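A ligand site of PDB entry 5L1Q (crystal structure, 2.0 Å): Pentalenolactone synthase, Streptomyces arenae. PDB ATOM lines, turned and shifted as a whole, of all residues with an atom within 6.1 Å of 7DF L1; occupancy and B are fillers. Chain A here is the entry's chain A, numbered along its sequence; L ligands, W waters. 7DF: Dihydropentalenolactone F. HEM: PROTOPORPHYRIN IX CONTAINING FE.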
ATOM      1  N   ARG A  77      -8.334   6.034  29.586  1.00  0.00           N
ATOM      2  CA  ARG A  77      -8.764   7.158  28.767  1.00  0.00           C
ATOM      3  C   ARG A  77      -8.593   8.488  29.484  1.00  0.00           C
ATOM      4  O   ARG A  77      -8.265   9.499  28.857  1.00  0.00           O
ATOM      5  CB  ARG A  77     -10.223   6.993  28.347  1.00  0.00           C
ATOM      6  CG  ARG A  77     -10.413   6.183  27.122  1.00  0.00           C
ATOM      7  CD  ARG A  77      -9.969   6.931  25.864  1.00  0.00           C
ATOM      8  NE  ARG A  77     -10.144   6.064  24.712  1.00  0.00           N
ATOM      9  CZ  ARG A  77      -9.762   6.342  23.473  1.00  0.00           C
ATOM     10  NH1 ARG A  77      -9.174   7.500  23.202  1.00  0.00           N
ATOM     11  NH2 ARG A  77      -9.990   5.471  22.505  1.00  0.00           N
ATOM     12  N   MET A  80      -4.997   9.424  29.200  1.00  0.00           N
ATOM     13  CA  MET A  80      -4.743   9.875  27.838  1.00  0.00           C
ATOM     14  C   MET A  80      -5.205  11.313  27.638  1.00  0.00           C
ATOM     15  O   MET A  80      -4.453  12.154  27.141  1.00  0.00           O
ATOM     16  CB  MET A  80      -5.444   8.958  26.844  1.00  0.00           C
ATOM     17  CG  MET A  80      -5.064   9.298  25.401  1.00  0.00           C
ATOM     18  SD  MET A  80      -5.537   7.987  24.263  1.00  0.00           S
ATOM     19  CE  MET A  80      -4.026   6.991  24.405  1.00  0.00           C
ATOM     20  N   MET A  84      -3.116  14.916  26.956  1.00  0.00           N
ATOM     21  CA  MET A  84      -3.393  15.769  25.801  1.00  0.00           C
ATOM     22  C   MET A  84      -3.998  17.117  26.183  1.00  0.00           C
ATOM     23  O   MET A  84      -4.486  17.828  25.299  1.00  0.00           O
ATOM     24  CB  MET A  84      -4.321  15.069  24.799  1.00  0.00           C
ATOM     25  CG  MET A  84      -3.631  13.937  24.029  1.00  0.00           C
ATOM     26  SD  MET A  84      -4.787  12.717  23.402  1.00  0.00           S
ATOM     27  CE  MET A  84      -5.098  13.564  21.827  1.00  0.00           C
ATOM     28  N   PHE A 174      -2.614   2.362  29.305  1.00  0.00           N
ATOM     29  CA  PHE A 174      -3.770   2.435  28.440  1.00  0.00           C
ATOM     30  C   PHE A 174      -4.581   1.154  28.449  1.00  0.00           C
ATOM     31  O   PHE A 174      -5.336   0.907  27.496  1.00  0.00           O
ATOM     32  CB  PHE A 174      -3.327   2.827  27.031  1.00  0.00           C
ATOM     33  CG  PHE A 174      -2.678   4.183  26.966  1.00  0.00           C
ATOM     34  CD1 PHE A 174      -3.138   5.228  27.748  1.00  0.00           C
ATOM     35  CD2 PHE A 174      -1.591   4.425  26.123  1.00  0.00           C
ATOM     36  CE1 PHE A 174      -2.528   6.495  27.696  1.00  0.00           C
ATOM     37  CE2 PHE A 174      -0.980   5.672  26.072  1.00  0.00           C
ATOM     38  CZ  PHE A 174      -1.449   6.707  26.858  1.00  0.00           C
ATOM     39  N   LEU A 234       4.657   8.145  26.321  1.00  0.00           N
ATOM     40  CA  LEU A 234       3.455   7.314  26.194  1.00  0.00           C
ATOM     41  C   LEU A 234       2.842   7.343  24.809  1.00  0.00           C
ATOM     42  O   LEU A 234       2.212   6.349  24.398  1.00  0.00           O
ATOM     43  CB  LEU A 234       2.423   7.742  27.248  1.00  0.00           C
ATOM     44  CG  LEU A 234       2.856   7.392  28.683  1.00  0.00           C
ATOM     45  CD1 LEU A 234       1.877   7.930  29.751  1.00  0.00           C
ATOM     46  CD2 LEU A 234       3.023   5.908  28.832  1.00  0.00           C
ATOM     47  N   PHE A 235       2.976   8.437  24.063  1.00  0.00           N
ATOM     48  CA  PHE A 235       2.511   8.479  22.681  1.00  0.00           C
ATOM     49  C   PHE A 235       3.613   8.174  21.675  1.00  0.00           C
ATOM     50  O   PHE A 235       3.305   7.935  20.496  1.00  0.00           O
ATOM     51  CB  PHE A 235       1.892   9.849  22.350  1.00  0.00           C
ATOM     52  CG  PHE A 235       0.784  10.282  23.298  1.00  0.00           C
ATOM     53  CD1 PHE A 235       0.039   9.349  24.009  1.00  0.00           C
ATOM     54  CD2 PHE A 235       0.495  11.636  23.463  1.00  0.00           C
ATOM     55  CE1 PHE A 235      -0.976   9.740  24.877  1.00  0.00           C
ATOM     56  CE2 PHE A 235      -0.507  12.047  24.334  1.00  0.00           C
ATOM     57  CZ  PHE A 235      -1.255  11.103  25.037  1.00  0.00           C
ATOM     58  N   THR A 239       2.448   3.227  19.379  1.00  0.00           N
ATOM     59  CA  THR A 239       1.715   3.290  18.110  1.00  0.00           C
ATOM     60  C   THR A 239       2.642   2.976  16.935  1.00  0.00           C
ATOM     61  O   THR A 239       2.215   2.333  15.968  1.00  0.00           O
ATOM     62  CB  THR A 239       1.071   4.676  17.948  1.00  0.00           C
ATOM     63  OG1 THR A 239       0.265   4.960  19.097  1.00  0.00           O
ATOM     64  CG2 THR A 239       0.173   4.708  16.708  1.00  0.00           C
ATOM     65  N   ARG A 243       2.563  -0.080  13.991  1.00  0.00           N
ATOM     66  CA  ARG A 243       2.592   0.125  12.542  1.00  0.00           C
ATOM     67  C   ARG A 243       3.676  -0.708  11.861  1.00  0.00           C
ATOM     68  O   ARG A 243       3.508  -1.095  10.695  1.00  0.00           O
ATOM     69  CB  ARG A 243       2.769   1.606  12.207  1.00  0.00           C
ATOM     70  CG  ARG A 243       1.575   2.498  12.627  1.00  0.00           C
ATOM     71  CD  ARG A 243       0.259   1.763  12.430  1.00  0.00           C
ATOM     72  NE  ARG A 243      -0.929   2.534  12.841  1.00  0.00           N
ATOM     73  CZ  ARG A 243      -1.383   2.646  14.088  1.00  0.00           C
ATOM     74  NH1 ARG A 243      -0.730   2.062  15.096  1.00  0.00           N
ATOM     75  NH2 ARG A 243      -2.491   3.353  14.349  1.00  0.00           N
ATOM     76  N   SER A 285     -10.717  -0.218  17.124  1.00  0.00           N
ATOM     77  CA  SER A 285     -11.207   0.831  18.022  1.00  0.00           C
ATOM     78  C   SER A 285     -10.206   1.969  18.147  1.00  0.00           C
ATOM     79  O   SER A 285     -10.593   3.107  18.451  1.00  0.00           O
ATOM     80  CB  SER A 285     -11.532   0.249  19.402  1.00  0.00           C
ATOM     81  OG  SER A 285     -12.571  -0.718  19.311  1.00  0.00           O
ATOM     82  N   ASN A 286      -8.915   1.687  17.932  1.00  0.00           N
ATOM     83  CA  ASN A 286      -7.913   2.741  17.948  1.00  0.00           C
ATOM     84  C   ASN A 286      -7.940   3.593  16.689  1.00  0.00           C
ATOM     85  O   ASN A 286      -7.310   4.661  16.658  1.00  0.00           O
ATOM     86  CB  ASN A 286      -6.504   2.146  18.146  1.00  0.00           C
ATOM     87  CG  ASN A 286      -6.150   1.139  17.069  1.00  0.00           C
ATOM     88  OD1 ASN A 286      -6.974   0.331  16.648  1.00  0.00           O
ATOM     89  ND2 ASN A 286      -4.905   1.197  16.603  1.00  0.00           N
ATOM     90  N   ALA A 287      -8.644   3.174  15.640  1.00  0.00           N
ATOM     91  CA  ALA A 287      -8.782   3.967  14.429  1.00  0.00           C
ATOM     92  C   ALA A 287      -9.983   4.905  14.502  1.00  0.00           C
ATOM     93  O   ALA A 287     -10.588   5.239  13.482  1.00  0.00           O
ATOM     94  CB  ALA A 287      -8.890   3.077  13.188  1.00  0.00           C
ATOM     95  N   LEU A 288     -10.365   5.307  15.711  1.00  0.00           N
ATOM     96  CA  LEU A 288     -11.418   6.283  15.944  1.00  0.00           C
ATOM     97  C   LEU A 288     -10.832   7.422  16.751  1.00  0.00           C
ATOM     98  O   LEU A 288     -10.219   7.190  17.809  1.00  0.00           O
ATOM     99  CB  LEU A 288     -12.586   5.647  16.700  1.00  0.00           C
ATOM    100  CG  LEU A 288     -13.272   4.396  16.138  1.00  0.00           C
ATOM    101  CD1 LEU A 288     -14.301   3.911  17.143  1.00  0.00           C
ATOM    102  CD2 LEU A 288     -13.927   4.676  14.798  1.00  0.00           C
ATOM    103  N   ILE A 289     -10.989   8.643  16.271  1.00  0.00           N
ATOM    104  CA  ILE A 289     -10.583   9.837  17.011  1.00  0.00           C
ATOM    105  C   ILE A 289     -11.824  10.379  17.718  1.00  0.00           C
ATOM    106  O   ILE A 289     -12.795  10.741  17.038  1.00  0.00           O
ATOM    107  CB  ILE A 289      -9.949  10.902  16.103  1.00  0.00           C
ATOM    108  CG1 ILE A 289      -8.604  10.397  15.555  1.00  0.00           C
ATOM    109  CG2 ILE A 289      -9.777  12.214  16.866  1.00  0.00           C
ATOM    110  CD1 ILE A 289      -7.844  11.447  14.741  1.00  0.00           C
ATOM    111  N   PRO A 290     -11.844  10.430  19.050  1.00  0.00           N
ATOM    112  CA  PRO A 290     -13.039  10.882  19.760  1.00  0.00           C
ATOM    113  C   PRO A 290     -13.061  12.382  19.984  1.00  0.00           C
ATOM    114  O   PRO A 290     -12.025  13.015  20.227  1.00  0.00           O
ATOM    115  CB  PRO A 290     -12.923  10.144  21.103  1.00  0.00           C
ATOM    116  CG  PRO A 290     -11.419  10.163  21.349  1.00  0.00           C
ATOM    117  CD  PRO A 290     -10.786   9.988  19.969  1.00  0.00           C
ATOM    118  N   ILE A 314     -11.081   7.503  11.352  1.00  0.00           N
ATOM    119  CA  ILE A 314      -9.998   7.741  10.411  1.00  0.00           C
ATOM    120  C   ILE A 314      -9.643   6.475   9.647  1.00  0.00           C
ATOM    121  O   ILE A 314      -9.235   6.536   8.483  1.00  0.00           O
ATOM    122  CB  ILE A 314      -8.758   8.325  11.147  1.00  0.00           C
ATOM    123  CG1 ILE A 314      -8.324   7.424  12.302  1.00  0.00           C
ATOM    124  CG2 ILE A 314      -9.046   9.770  11.599  1.00  0.00           C
ATOM    125  CD1 ILE A 314      -7.068   7.910  13.068  1.00  0.00           C
ATOM    126  N   ALA A 342      -4.238   8.840   8.998  1.00  0.00           N
ATOM    127  CA  ALA A 342      -3.733   7.998  10.092  1.00  0.00           C
ATOM    128  C   ALA A 342      -3.065   8.809  11.199  1.00  0.00           C
ATOM    129  O   ALA A 342      -2.999   8.343  12.330  1.00  0.00           O
ATOM    130  CB  ALA A 342      -2.748   6.950   9.572  1.00  0.00           C
ATOM    131  N   ILE A 390      -5.983   0.848  24.584  1.00  0.00           N
ATOM    132  CA  ILE A 390      -6.396   1.939  23.690  1.00  0.00           C
ATOM    133  C   ILE A 390      -5.598   1.870  22.390  1.00  0.00           C
ATOM    134  O   ILE A 390      -6.136   2.122  21.305  1.00  0.00           O
ATOM    135  CB  ILE A 390      -6.235   3.318  24.366  1.00  0.00           C
ATOM    136  CG1 ILE A 390      -7.173   3.472  25.565  1.00  0.00           C
ATOM    137  CG2 ILE A 390      -6.576   4.407  23.368  1.00  0.00           C
ATOM    138  CD1 ILE A 390      -6.857   4.710  26.415  1.00  0.00           C
ATOM    139  N   THR A 391      -4.323   1.509  22.477  1.00  0.00           N
ATOM    140  CA  THR A 391      -3.448   1.415  21.308  1.00  0.00           C
ATOM    141  C   THR A 391      -3.475   0.038  20.631  1.00  0.00           C
ATOM    142  O   THR A 391      -2.718  -0.170  19.673  1.00  0.00           O
ATOM    143  CB  THR A 391      -2.010   1.789  21.706  1.00  0.00           C
ATOM    144  OG1 THR A 391      -1.686   1.129  22.929  1.00  0.00           O
ATOM    145  CG2 THR A 391      -1.893   3.310  21.938  1.00  0.00           C
ATOM    146  N   GLY A 392      -4.311  -0.897  21.075  1.00  0.00           N
ATOM    147  CA  GLY A 392      -4.442  -2.176  20.368  1.00  0.00           C
ATOM    148  C   GLY A 392      -3.123  -2.924  20.282  1.00  0.00           C
ATOM    149  O   GLY A 392      -2.400  -3.067  21.268  1.00  0.00           O
HETATM  150  C1  7DF L   1      -2.770   9.146  19.114  1.00  0.00           C
HETATM  151  C2  7DF L   1      -2.847   8.833  20.626  1.00  0.00           C
HETATM  152  C3  7DF L   1      -4.348   8.460  20.788  1.00  0.00           C
HETATM  153  C4  7DF L   1      -4.722   7.654  19.487  1.00  0.00           C
HETATM  154  C5  7DF L   1      -4.488   6.118  19.549  1.00  0.00           C
HETATM  155  C6  7DF L   1      -4.059   5.818  18.099  1.00  0.00           C
HETATM  156  C9  7DF L   1      -6.217   7.933  19.167  1.00  0.00           C
HETATM  157  C10 7DF L   1      -6.736   7.983  17.745  1.00  0.00           C
HETATM  158  C11 7DF L   1      -7.031   7.422  20.198  1.00  0.00           C
HETATM  159  C15 7DF L   1      -2.531  10.118  21.408  1.00  0.00           C
HETATM  160  C14 7DF L   1      -1.877   7.732  21.093  1.00  0.00           C
HETATM  161  C12 7DF L   1      -5.800   5.353  19.846  1.00  0.00           C
HETATM  162  C7  7DF L   1      -2.964   6.857  17.946  1.00  0.00           C
HETATM  163  C13 7DF L   1      -3.520   4.405  17.855  1.00  0.00           C
HETATM  164  C8  7DF L   1      -3.715   8.136  18.393  1.00  0.00           C
HETATM  165  O4  7DF L   1      -2.917   3.837  18.786  1.00  0.00           O
HETATM  166  O2  7DF L   1      -7.864   8.144  20.757  1.00  0.00           O
HETATM  167  O5  7DF L   1      -3.686   3.909  16.716  1.00  0.00           O
HETATM  168  O3  7DF L   1      -6.771   6.130  20.618  1.00  0.00           O
HETATM  169  O1  7DF L   1      -6.616   9.177  18.585  1.00  0.00           O
HETATM  170  CHA HEM L   2      -1.390  12.824  18.272  1.00  0.00           C
HETATM  171  CHB HEM L   2      -1.136   8.924  15.377  1.00  0.00           C
HETATM  172  CHC HEM L   2       3.546   8.402  16.413  1.00  0.00           C
HETATM  173  CHD HEM L   2       3.321  12.207  19.410  1.00  0.00           C
HETATM  174  C1A HEM L   2      -1.732  11.855  17.367  1.00  0.00           C
HETATM  175  C2A HEM L   2      -3.027  11.703  16.718  1.00  0.00           C
HETATM  176  C3A HEM L   2      -2.938  10.623  15.913  1.00  0.00           C
HETATM  177  C4A HEM L   2      -1.602  10.054  16.034  1.00  0.00           C
HETATM  178  CMA HEM L   2      -4.063  10.024  15.029  1.00  0.00           C
HETATM  179  CAA HEM L   2      -4.263  12.645  16.899  1.00  0.00           C
HETATM  180  CBA HEM L   2      -5.195  12.237  18.052  1.00  0.00           C
HETATM  181  CGA HEM L   2      -6.395  13.146  18.127  1.00  0.00           C
HETATM  182  O1A HEM L   2      -6.590  14.009  17.222  1.00  0.00           O
HETATM  183  O2A HEM L   2      -7.201  13.003  19.104  1.00  0.00           O
HETATM  184  C1B HEM L   2       0.136   8.419  15.371  1.00  0.00           C
HETATM  185  C2B HEM L   2       0.664   7.305  14.592  1.00  0.00           C
HETATM  186  C3B HEM L   2       1.960   7.174  14.916  1.00  0.00           C
HETATM  187  C4B HEM L   2       2.293   8.205  15.868  1.00  0.00           C
HETATM  188  CMB HEM L   2      -0.141   6.426  13.592  1.00  0.00           C
HETATM  189  CAB HEM L   2       3.043   6.187  14.411  1.00  0.00           C
HETATM  190  CBB HEM L   2       3.020   5.600  13.202  1.00  0.00           C
HETATM  191  C1C HEM L   2       3.924   9.420  17.253  1.00  0.00           C
HETATM  192  C2C HEM L   2       5.282   9.712  17.651  1.00  0.00           C
HETATM  193  C3C HEM L   2       5.229  10.764  18.483  1.00  0.00           C
HETATM  194  C4C HEM L   2       3.835  11.163  18.646  1.00  0.00           C
HETATM  195  CMC HEM L   2       6.519   8.898  17.138  1.00  0.00           C
HETATM  196  CAC HEM L   2       6.401  11.488  19.214  1.00  0.00           C
HETATM  197  CBC HEM L   2       7.613  10.931  19.443  1.00  0.00           C
HETATM  198  C1D HEM L   2       2.018  12.670  19.400  1.00  0.00           C
HETATM  199  C2D HEM L   2       1.474  13.697  20.259  1.00  0.00           C
HETATM  200  C3D HEM L   2       0.173  13.870  19.968  1.00  0.00           C
HETATM  201  C4D HEM L   2      -0.162  12.944  18.900  1.00  0.00           C
HETATM  202  CMD HEM L   2       2.303  14.439  21.331  1.00  0.00           C
HETATM  203  CAD HEM L   2      -0.819  14.852  20.608  1.00  0.00           C
HETATM  204  CBD HEM L   2      -1.050  16.055  19.672  1.00  0.00           C
HETATM  205  CGD HEM L   2      -2.172  16.931  20.191  1.00  0.00           C
HETATM  206  O1D HEM L   2      -2.149  18.150  19.867  1.00  0.00           O
HETATM  207  O2D HEM L   2      -3.064  16.438  20.936  1.00  0.00           O
HETATM  208  NA  HEM L   2      -0.895  10.838  16.931  1.00  0.00           N
HETATM  209  NB  HEM L   2       1.159   8.932  16.142  1.00  0.00           N
HETATM  210  NC  HEM L   2       3.062  10.314  17.886  1.00  0.00           N
HETATM  211  ND  HEM L   2       0.990  12.236  18.594  1.00  0.00           N
HETATM  212 FE   HEM L   2       1.135  10.674  17.221  1.00  0.00          FE
HETATM  213  O   HOH W   1      -7.567  10.875  20.888  1.00  0.00           O
HETATM  214  O   HOH W   2      -9.928   5.353  19.909  1.00  0.00           O
HETATM  215  O   HOH W   3      -5.182   4.991  14.902  1.00  0.00           O
HETATM  216  O   HOH W   4       0.877   8.167  19.001  1.00  0.00           O
HETATM  217  O   HOH W   5      -1.608   1.631  17.704  1.00  0.00           O
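N of Ile 390 is in hydrogen-bond range of O of Phe 174.
The guanidinium group of Arg 243 lies within hydrogen-bond range of the backbone carbonyl oxygen of Thr 239.
The guanidinium group (NH1) of Arg 77 is in hydrogen-bond range of an oxygen (O2) of 7DF L1, at 2.8 Å.
An oxygen (O4) of 7DF L1 lies within hydrogen-bond range of the side-chain hydroxyl (OG1) of Thr 239 (3.4 Å).
An oxygen (O5) of 7DF L1 sits at hydrogen-bond distance from the side-chain amide nitrogen (ND2) of Asn 286 (3.0 Å).
An oxygen (O5) of 7DF L1 is in salt-bridge range of the guanidinium group (NH2) of Arg 243, 2.7 Å away.
Water W3 lies within hydrogen-bond range of O5 of 7DF L1 (2.6 Å), O of Asn 286 (2.8 Å) and NH2 of Arg 243 (3.2 Å).
Water W1 bridges an oxygen (O2) of 7DF L1 (2.8 Å) and an oxygen (O2A) of HEM L2 (2.8 Å).
Water W5 lies within hydrogen-bond range of an oxygen (O4) of 7DF L1 (2.8 Å), the guanidinium group (NH1) of Arg 243 (2.8 Å) and the backbone carbonyl oxygen (O) of Thr 391 (2.9 Å).
Water W4 bridges the backbone carbonyl oxygen of Phe 235 and the side-chain hydroxyl of Thr 239.
Merely in contact with 7DF L1: Ile 390, Thr 391, Pro 290, Leu 288, Met 80, Phe 235, Ile 289 and Met 84.
Hydrophobic or aromatic side chains that line 7DF L1: Met 80, Met 84, Phe 235, Ile 289, Pro 290 and Ile 390.
Of the 19 residues printed, 12 come within 4 Å of 7DF L1.
The nearest printed residue that does not touch 7DF L1 is Ile 314 (4.7 Å).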
